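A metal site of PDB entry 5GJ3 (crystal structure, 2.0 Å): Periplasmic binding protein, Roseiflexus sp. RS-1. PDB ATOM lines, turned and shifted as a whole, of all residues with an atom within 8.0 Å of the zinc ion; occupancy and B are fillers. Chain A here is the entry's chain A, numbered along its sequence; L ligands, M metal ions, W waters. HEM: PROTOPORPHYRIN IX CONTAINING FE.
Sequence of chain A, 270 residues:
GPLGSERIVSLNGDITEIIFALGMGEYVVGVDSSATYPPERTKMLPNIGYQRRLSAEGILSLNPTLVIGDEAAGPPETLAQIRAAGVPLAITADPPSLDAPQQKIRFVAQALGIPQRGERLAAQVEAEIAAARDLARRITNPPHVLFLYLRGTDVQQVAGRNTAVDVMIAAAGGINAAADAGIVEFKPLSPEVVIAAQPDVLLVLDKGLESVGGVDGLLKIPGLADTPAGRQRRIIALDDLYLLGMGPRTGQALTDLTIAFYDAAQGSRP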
ATOM      1  N   LEU A  11      -3.305 -25.938   0.995  1.00  0.00           N
ATOM      2  CA  LEU A  11      -2.072 -26.181   1.744  1.00  0.00           C
ATOM      3  C   LEU A  11      -1.056 -24.989   1.854  1.00  0.00           C
ATOM      4  O   LEU A  11      -0.097 -25.075   2.637  1.00  0.00           O
ATOM      5  CB  LEU A  11      -1.339 -27.447   1.194  1.00  0.00           C
ATOM      6  CG  LEU A  11      -2.237 -28.706   1.121  1.00  0.00           C
ATOM      7  CD1 LEU A  11      -1.379 -29.812   0.522  1.00  0.00           C
ATOM      8  CD2 LEU A  11      -2.702 -29.095   2.525  1.00  0.00           C
ATOM      9  N   ASN A  12      -1.248 -23.954   1.064  1.00  0.00           N
ATOM     10  CA  ASN A  12      -0.265 -22.862   1.013  1.00  0.00           C
ATOM     11  C   ASN A  12      -0.993 -21.558   0.979  1.00  0.00           C
ATOM     12  O   ASN A  12      -2.049 -21.449   0.340  1.00  0.00           O
ATOM     13  CB  ASN A  12       0.670 -22.963  -0.212  1.00  0.00           C
ATOM     14  CG  ASN A  12       1.287 -24.300  -0.333  1.00  0.00           C
ATOM     15  OD1 ASN A  12       0.735 -25.209  -0.940  1.00  0.00           O
ATOM     16  ND2 ASN A  12       2.409 -24.475   0.321  1.00  0.00           N
ATOM     17  N   GLY A  13      -0.436 -20.555   1.670  1.00  0.00           N
ATOM     18  CA  GLY A  13      -1.017 -19.208   1.638  1.00  0.00           C
ATOM     19  C   GLY A  13      -1.291 -18.588   0.293  1.00  0.00           C
ATOM     20  O   GLY A  13      -2.317 -17.945   0.120  1.00  0.00           O
ATOM     21  N   ASP A  14      -0.377 -18.755  -0.682  1.00  0.00           N
ATOM     22  CA  ASP A  14      -0.591 -18.216  -2.025  1.00  0.00           C
ATOM     23  C   ASP A  14      -1.697 -18.921  -2.881  1.00  0.00           C
ATOM     24  O   ASP A  14      -2.473 -18.267  -3.633  1.00  0.00           O
ATOM     25  CB  ASP A  14       0.754 -18.142  -2.791  1.00  0.00           C
ATOM     26  CG  ASP A  14       1.476 -19.495  -2.913  1.00  0.00           C
ATOM     27  OD1 ASP A  14       1.226 -20.440  -2.116  1.00  0.00           O
ATOM     28  OD2 ASP A  14       2.348 -19.620  -3.832  1.00  0.00           O
ATOM     29  N   ILE A  15      -1.815 -20.239  -2.707  1.00  0.00           N
ATOM     30  CA  ILE A  15      -2.935 -21.009  -3.284  1.00  0.00           C
ATOM     31  C   ILE A  15      -4.276 -20.561  -2.692  1.00  0.00           C
ATOM     32  O   ILE A  15      -5.247 -20.311  -3.420  1.00  0.00           O
ATOM     33  CB  ILE A  15      -2.698 -22.504  -3.045  1.00  0.00           C
ATOM     34  CG1 ILE A  15      -1.363 -22.895  -3.706  1.00  0.00           C
ATOM     35  CG2 ILE A  15      -3.877 -23.296  -3.612  1.00  0.00           C
ATOM     36  CD1 ILE A  15      -1.303 -22.653  -5.215  1.00  0.00           C
ATOM     37  N   ILE A  18      -5.336 -17.330  -4.082  1.00  0.00           N
ATOM     38  CA  ILE A  18      -5.769 -17.468  -5.450  1.00  0.00           C
ATOM     39  C   ILE A  18      -7.241 -18.054  -5.452  1.00  0.00           C
ATOM     40  O   ILE A  18      -8.034 -17.667  -6.282  1.00  0.00           O
ATOM     41  CB  ILE A  18      -4.837 -18.439  -6.246  1.00  0.00           C
ATOM     42  CG1 ILE A  18      -3.510 -17.742  -6.615  1.00  0.00           C
ATOM     43  CG2 ILE A  18      -5.567 -18.918  -7.511  1.00  0.00           C
ATOM     44  CD1 ILE A  18      -2.457 -18.730  -7.095  1.00  0.00           C
ATOM     45  N   SER A  34       0.363 -19.788   6.952  1.00  0.00           N
ATOM     46  CA  SER A  34       0.820 -18.683   6.093  1.00  0.00           C
ATOM     47  C   SER A  34      -0.336 -18.048   5.299  1.00  0.00           C
ATOM     48  O   SER A  34      -0.115 -17.138   4.493  1.00  0.00           O
ATOM     49  CB  SER A  34       1.926 -19.151   5.124  1.00  0.00           C
ATOM     50  OG  SER A  34       1.334 -19.958   4.098  1.00  0.00           O
ATOM     51  N   GLN A  51       2.484 -24.574   6.251  1.00  0.00           N
ATOM     52  CA  GLN A  51       2.613 -25.217   4.895  1.00  0.00           C
ATOM     53  C   GLN A  51       3.686 -26.305   4.737  1.00  0.00           C
ATOM     54  O   GLN A  51       3.465 -27.264   4.010  1.00  0.00           O
ATOM     55  CB  GLN A  51       2.744 -24.167   3.771  1.00  0.00           C
ATOM     56  CG  GLN A  51       4.076 -23.374   3.773  1.00  0.00           C
ATOM     57  CD  GLN A  51       4.018 -22.156   2.864  1.00  0.00           C
ATOM     58  OE1 GLN A  51       3.278 -22.143   1.849  1.00  0.00           O
ATOM     59  NE2 GLN A  51       4.781 -21.124   3.216  1.00  0.00           N
ATOM     60  N   ARG A  52       4.823 -26.161   5.437  1.00  0.00           N
ATOM     61  CA  ARG A  52       5.925 -27.153   5.362  1.00  0.00           C
ATOM     62  C   ARG A  52       5.899 -28.122   6.530  1.00  0.00           C
ATOM     63  O   ARG A  52       6.729 -29.006   6.622  1.00  0.00           O
ATOM     64  CB  ARG A  52       7.289 -26.432   5.422  1.00  0.00           C
ATOM     65  CG  ARG A  52       7.508 -25.464   4.251  1.00  0.00           C
ATOM     66  CD  ARG A  52       8.978 -25.028   4.189  1.00  0.00           C
ATOM     67  NE  ARG A  52       9.371 -24.589   2.845  1.00  0.00           N
ATOM     68  CZ  ARG A  52       8.885 -23.510   2.212  1.00  0.00           C
ATOM     69  NH1 ARG A  52       7.949 -22.739   2.752  1.00  0.00           N
ATOM     70  NH2 ARG A  52       9.343 -23.195   1.010  1.00  0.00           N
ATOM     71  N   GLY A  69      -2.405 -27.689  -3.224  1.00  0.00           N
ATOM     72  CA  GLY A  69      -1.209 -26.938  -2.699  1.00  0.00           C
ATOM     73  C   GLY A  69      -0.144 -26.849  -3.792  1.00  0.00           C
ATOM     74  O   GLY A  69      -0.391 -27.210  -4.960  1.00  0.00           O
ATOM     75  N   ASP A  70       1.024 -26.346  -3.450  1.00  0.00           N
ATOM     76  CA  ASP A  70       2.074 -26.303  -4.441  1.00  0.00           C
ATOM     77  C   ASP A  70       3.300 -26.906  -3.796  1.00  0.00           C
ATOM     78  O   ASP A  70       3.214 -27.509  -2.686  1.00  0.00           O
ATOM     79  CB  ASP A  70       2.263 -24.896  -4.991  1.00  0.00           C
ATOM     80  CG  ASP A  70       2.801 -23.911  -3.959  1.00  0.00           C
ATOM     81  OD1 ASP A  70       3.458 -24.297  -2.952  1.00  0.00           O
ATOM     82  OD2 ASP A  70       2.556 -22.724  -4.160  1.00  0.00           O
ATOM     83  N   GLU A  71       4.425 -26.844  -4.493  1.00  0.00           N
ATOM     84  CA  GLU A  71       5.631 -27.586  -4.088  1.00  0.00           C
ATOM     85  C   GLU A  71       6.192 -27.245  -2.706  1.00  0.00           C
ATOM     86  O   GLU A  71       6.953 -28.044  -2.171  1.00  0.00           O
ATOM     87  CB  GLU A  71       6.771 -27.475  -5.147  1.00  0.00           C
ATOM     88  CG  GLU A  71       7.279 -26.052  -5.361  1.00  0.00           C
ATOM     89  CD  GLU A  71       8.402 -25.971  -6.408  1.00  0.00           C
ATOM     90  OE1 GLU A  71       8.162 -25.731  -7.628  1.00  0.00           O
ATOM     91  OE2 GLU A  71       9.561 -26.176  -5.993  1.00  0.00           O
ATOM     92  N   ALA A  72       5.827 -26.096  -2.124  1.00  0.00           N
ATOM     93  CA  ALA A  72       6.220 -25.793  -0.740  1.00  0.00           C
ATOM     94  C   ALA A  72       5.511 -26.683   0.310  1.00  0.00           C
ATOM     95  O   ALA A  72       5.996 -26.762   1.447  1.00  0.00           O
ATOM     96  CB  ALA A  72       6.026 -24.314  -0.398  1.00  0.00           C
ATOM     97  N   ALA A  73       4.397 -27.327  -0.054  1.00  0.00           N
ATOM     98  CA  ALA A  73       3.619 -28.090   0.903  1.00  0.00           C
ATOM     99  C   ALA A  73       4.382 -29.315   1.348  1.00  0.00           C
ATOM    100  O   ALA A  73       4.942 -30.068   0.529  1.00  0.00           O
ATOM    101  CB  ALA A  73       2.257 -28.552   0.289  1.00  0.00           C
ATOM    102  N   THR A  92       0.943 -28.246  -7.471  1.00  0.00           N
ATOM    103  CA  THR A  92       1.582 -27.594  -8.605  1.00  0.00           C
ATOM    104  C   THR A  92       3.007 -27.072  -8.325  1.00  0.00           C
ATOM    105  O   THR A  92       3.425 -26.907  -7.172  1.00  0.00           O
ATOM    106  CB  THR A  92       0.681 -26.421  -9.079  1.00  0.00           C
ATOM    107  OG1 THR A  92       1.081 -26.029 -10.399  1.00  0.00           O
ATOM    108  CG2 THR A  92       0.795 -25.220  -8.107  1.00  0.00           C
ATOM    109  N   ALA A  93       3.775 -26.804  -9.381  1.00  0.00           N
ATOM    110  CA  ALA A  93       5.107 -26.186  -9.223  1.00  0.00           C
ATOM    111  C   ALA A  93       4.959 -24.755  -8.727  1.00  0.00           C
ATOM    112  O   ALA A  93       3.923 -24.101  -8.959  1.00  0.00           O
ATOM    113  CB  ALA A  93       5.878 -26.190 -10.550  1.00  0.00           C
ATOM    114  N   ASP A  94       5.995 -24.252  -8.071  1.00  0.00           N
ATOM    115  CA  ASP A  94       6.012 -22.823  -7.714  1.00  0.00           C
ATOM    116  C   ASP A  94       7.428 -22.254  -7.883  1.00  0.00           C
ATOM    117  O   ASP A  94       8.052 -21.949  -6.868  1.00  0.00           O
ATOM    118  CB  ASP A  94       5.556 -22.643  -6.255  1.00  0.00           C
ATOM    119  CG  ASP A  94       5.320 -21.164  -5.857  1.00  0.00           C
ATOM    120  OD1 ASP A  94       5.297 -20.238  -6.737  1.00  0.00           O
ATOM    121  OD2 ASP A  94       5.149 -20.956  -4.641  1.00  0.00           O
ATOM    122  N   PRO A  95       7.942 -22.168  -9.134  1.00  0.00           N
ATOM    123  CA  PRO A  95       9.281 -21.671  -9.442  1.00  0.00           C
ATOM    124  C   PRO A  95       9.446 -20.170  -9.052  1.00  0.00           C
ATOM    125  O   PRO A  95       8.449 -19.434  -8.983  1.00  0.00           O
ATOM    126  CB  PRO A  95       9.359 -21.851 -10.969  1.00  0.00           C
ATOM    127  CG  PRO A  95       7.916 -21.673 -11.414  1.00  0.00           C
ATOM    128  CD  PRO A  95       7.198 -22.494 -10.364  1.00  0.00           C
ATOM    129  N   ALA A 100       5.190 -17.819 -12.600  1.00  0.00           N
ATOM    130  CA  ALA A 100       4.493 -18.573 -11.527  1.00  0.00           C
ATOM    131  C   ALA A 100       3.037 -18.090 -11.225  1.00  0.00           C
ATOM    132  O   ALA A 100       2.153 -18.949 -11.080  1.00  0.00           O
ATOM    133  CB  ALA A 100       5.336 -18.627 -10.241  1.00  0.00           C
ATOM    134  N   LYS A 104       0.051 -20.855 -11.447  1.00  0.00           N
ATOM    135  CA  LYS A 104      -0.703 -21.278 -10.252  1.00  0.00           C
ATOM    136  C   LYS A 104      -2.192 -20.961 -10.387  1.00  0.00           C
ATOM    137  O   LYS A 104      -3.081 -21.751  -9.917  1.00  0.00           O
ATOM    138  CB  LYS A 104      -0.116 -20.636  -8.979  1.00  0.00           C
ATOM    139  CG  LYS A 104       1.254 -21.229  -8.613  1.00  0.00           C
ATOM    140  CD  LYS A 104       1.815 -20.609  -7.314  1.00  0.00           C
ATOM    141  CE  LYS A 104       2.232 -19.184  -7.430  1.00  0.00           C
ATOM    142  NZ  LYS A 104       2.936 -18.630  -6.194  1.00  0.00           N
ATOM    143  N   LEU A 241       3.380 -12.244   2.346  1.00  0.00           N
ATOM    144  CA  LEU A 241       2.631 -12.906   1.274  1.00  0.00           C
ATOM    145  C   LEU A 241       2.520 -11.959   0.020  1.00  0.00           C
ATOM    146  O   LEU A 241       2.598 -12.388  -1.119  1.00  0.00           O
ATOM    147  CB  LEU A 241       1.233 -13.359   1.781  1.00  0.00           C
ATOM    148  CG  LEU A 241       0.363 -14.251   0.881  1.00  0.00           C
ATOM    149  CD1 LEU A 241       1.085 -15.492   0.341  1.00  0.00           C
ATOM    150  CD2 LEU A 241      -0.914 -14.655   1.619  1.00  0.00           C
ATOM    151  N   LEU A 244       6.212 -11.728  -1.618  1.00  0.00           N
ATOM    152  CA  LEU A 244       6.884 -12.974  -1.971  1.00  0.00           C
ATOM    153  C   LEU A 244       5.980 -14.133  -2.460  1.00  0.00           C
ATOM    154  O   LEU A 244       6.496 -15.135  -2.987  1.00  0.00           O
ATOM    155  CB  LEU A 244       7.714 -13.462  -0.774  1.00  0.00           C
ATOM    156  CG  LEU A 244       8.811 -12.503  -0.307  1.00  0.00           C
ATOM    157  CD1 LEU A 244       9.417 -13.121   0.939  1.00  0.00           C
ATOM    158  CD2 LEU A 244       9.893 -12.358  -1.396  1.00  0.00           C
ATOM    159  N   GLY A 245       4.653 -13.977  -2.308  1.00  0.00           N
ATOM    160  CA  GLY A 245       3.669 -14.982  -2.778  1.00  0.00           C
ATOM    161  C   GLY A 245       3.587 -15.346  -4.273  1.00  0.00           C
ATOM    162  O   GLY A 245       3.154 -16.461  -4.614  1.00  0.00           O
ATOM    163  N   MET A 246       4.025 -14.458  -5.170  1.00  0.00           N
ATOM    164  CA  MET A 246       3.935 -14.782  -6.608  1.00  0.00           C
ATOM    165  C   MET A 246       2.498 -15.202  -6.994  1.00  0.00           C
ATOM    166  O   MET A 246       2.236 -16.235  -7.622  1.00  0.00           O
ATOM    167  CB  MET A 246       4.996 -15.805  -7.030  1.00  0.00           C
ATOM    168  CG  MET A 246       6.408 -15.204  -7.033  1.00  0.00           C
ATOM    169  SD  MET A 246       6.619 -13.824  -8.211  1.00  0.00           S
ATOM    170  CE  MET A 246       8.419 -13.813  -8.255  1.00  0.00           C
ATOM    171  N   GLY A 247       1.564 -14.382  -6.536  1.00  0.00           N
ATOM    172  CA  GLY A 247       0.156 -14.671  -6.695  1.00  0.00           C
ATOM    173  C   GLY A 247      -0.524 -13.552  -7.428  1.00  0.00           C
ATOM    174  O   GLY A 247       0.129 -12.851  -8.203  1.00  0.00           O
HETATM  175  CHA HEM L   1       8.174 -20.666   9.027  1.00  0.00           C
HETATM  176  CHB HEM L   1       5.264 -17.792   6.384  1.00  0.00           C
HETATM  177  CHC HEM L   1       8.244 -18.754   2.618  1.00  0.00           C
HETATM  178  CHD HEM L   1      10.753 -22.017   5.190  1.00  0.00           C
HETATM  179  C1A HEM L   1       7.182 -19.796   8.631  1.00  0.00           C
HETATM  180  C2A HEM L   1       6.159 -19.367   9.502  1.00  0.00           C
HETATM  181  C3A HEM L   1       5.301 -18.579   8.794  1.00  0.00           C
HETATM  182  C4A HEM L   1       5.833 -18.501   7.459  1.00  0.00           C
HETATM  183  CMA HEM L   1       4.034 -17.897   9.321  1.00  0.00           C
HETATM  184  CAA HEM L   1       6.046 -19.787  10.957  1.00  0.00           C
HETATM  185  CBA HEM L   1       5.514 -21.243  10.953  1.00  0.00           C
HETATM  186  CGA HEM L   1       5.771 -21.996  12.238  1.00  0.00           C
HETATM  187  O1A HEM L   1       6.611 -21.572  13.034  1.00  0.00           O
HETATM  188  O2A HEM L   1       5.188 -23.072  12.512  1.00  0.00           O
HETATM  189  C1B HEM L   1       5.869 -17.776   5.106  1.00  0.00           C
HETATM  190  C2B HEM L   1       5.425 -16.971   3.994  1.00  0.00           C
HETATM  191  C3B HEM L   1       6.283 -17.217   2.947  1.00  0.00           C
HETATM  192  C4B HEM L   1       7.234 -18.226   3.441  1.00  0.00           C
HETATM  193  CMB HEM L   1       4.283 -15.987   3.998  1.00  0.00           C
HETATM  194  CAB HEM L   1       6.303 -16.677   1.560  1.00  0.00           C
HETATM  195  CBB HEM L   1       5.173 -16.195   0.998  1.00  0.00           C
HETATM  196  C1C HEM L   1       9.211 -19.659   2.970  1.00  0.00           C
HETATM  197  C2C HEM L   1      10.322 -20.031   2.184  1.00  0.00           C
HETATM  198  C3C HEM L   1      11.047 -20.977   2.926  1.00  0.00           C
HETATM  199  C4C HEM L   1      10.366 -21.142   4.181  1.00  0.00           C
HETATM  200  CMC HEM L   1      10.603 -19.474   0.785  1.00  0.00           C
HETATM  201  CAC HEM L   1      12.298 -21.697   2.543  1.00  0.00           C
HETATM  202  CBC HEM L   1      12.961 -21.449   1.416  1.00  0.00           C
HETATM  203  C1D HEM L   1      10.227 -21.839   6.468  1.00  0.00           C
HETATM  204  C2D HEM L   1      10.775 -22.615   7.605  1.00  0.00           C
HETATM  205  C3D HEM L   1      10.062 -22.241   8.668  1.00  0.00           C
HETATM  206  C4D HEM L   1       9.089 -21.252   8.177  1.00  0.00           C
HETATM  207  CMD HEM L   1      11.930 -23.604   7.567  1.00  0.00           C
HETATM  208  CAD HEM L   1      10.217 -22.765  10.092  1.00  0.00           C
HETATM  209  CBD HEM L   1       8.998 -23.749  10.289  1.00  0.00           C
HETATM  210  CGD HEM L   1       9.222 -25.194   9.855  1.00  0.00           C
HETATM  211  O1D HEM L   1      10.372 -25.665   9.774  1.00  0.00           O
HETATM  212  O2D HEM L   1       8.265 -25.985   9.611  1.00  0.00           O
HETATM  213  NA  HEM L   1       6.936 -19.336   7.390  1.00  0.00           N
HETATM  214  NB  HEM L   1       6.889 -18.528   4.702  1.00  0.00           N
HETATM  215  NC  HEM L   1       9.242 -20.345   4.156  1.00  0.00           N
HETATM  216  ND  HEM L   1       9.162 -21.052   6.835  1.00  0.00           N
HETATM  217 FE   HEM L   1       8.046 -19.860   5.804  1.00  0.00          FE
HETATM  218 ZN    ZN M   1       3.629 -21.221  -3.294  1.00  0.00          ZN
HETATM  219  O   HOH W   1       4.014 -21.722  -1.443  1.00  0.00           O
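The zinc ion is bound by water W1 (2.0 Å), the side-chain carboxylate (OD2) of Asp 70 (2.0 Å), the side-chain carboxylate (OD2) of Asp 94 (2.0 Å) and the side-chain carboxylate (OD2) of Asp 14 (2.1 Å).
Slightly farther from the zinc ion lies OD1 of Asp 14 (2.8 Å).
OD1 of Asn 12 sits at hydrogen-bond distance from N of Asp 70.
The side-chain carboxylate (OD1) of Asp 70 sits at hydrogen-bond distance from the backbone NH (N) of Ala 72 (3.1 Å).
The side-chain carboxylate of Asp 94 is in salt-bridge range of the side-chain amino group of Lys 104, at 2.9 Å.
OE1 of Glu 71 sits at hydrogen-bond distance from N of Asp 94, 2.7 Å away.
The side-chain carboxylate of Asp 14 lies close to the side-chain amino group of Lys 104 (2.6 Å).
The side-chain amino group (NZ) of Lys 104 is in hydrogen-bond range of the backbone carbonyl oxygen (O) of Gly 245, 2.7 Å away.
O of Met 246 sits at hydrogen-bond distance from NZ of Lys 104 (2.9 Å).
Lys 104 touches the zinc ion.
Of the 25 residues printed, 4 come within 4 Å of the zinc ion.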
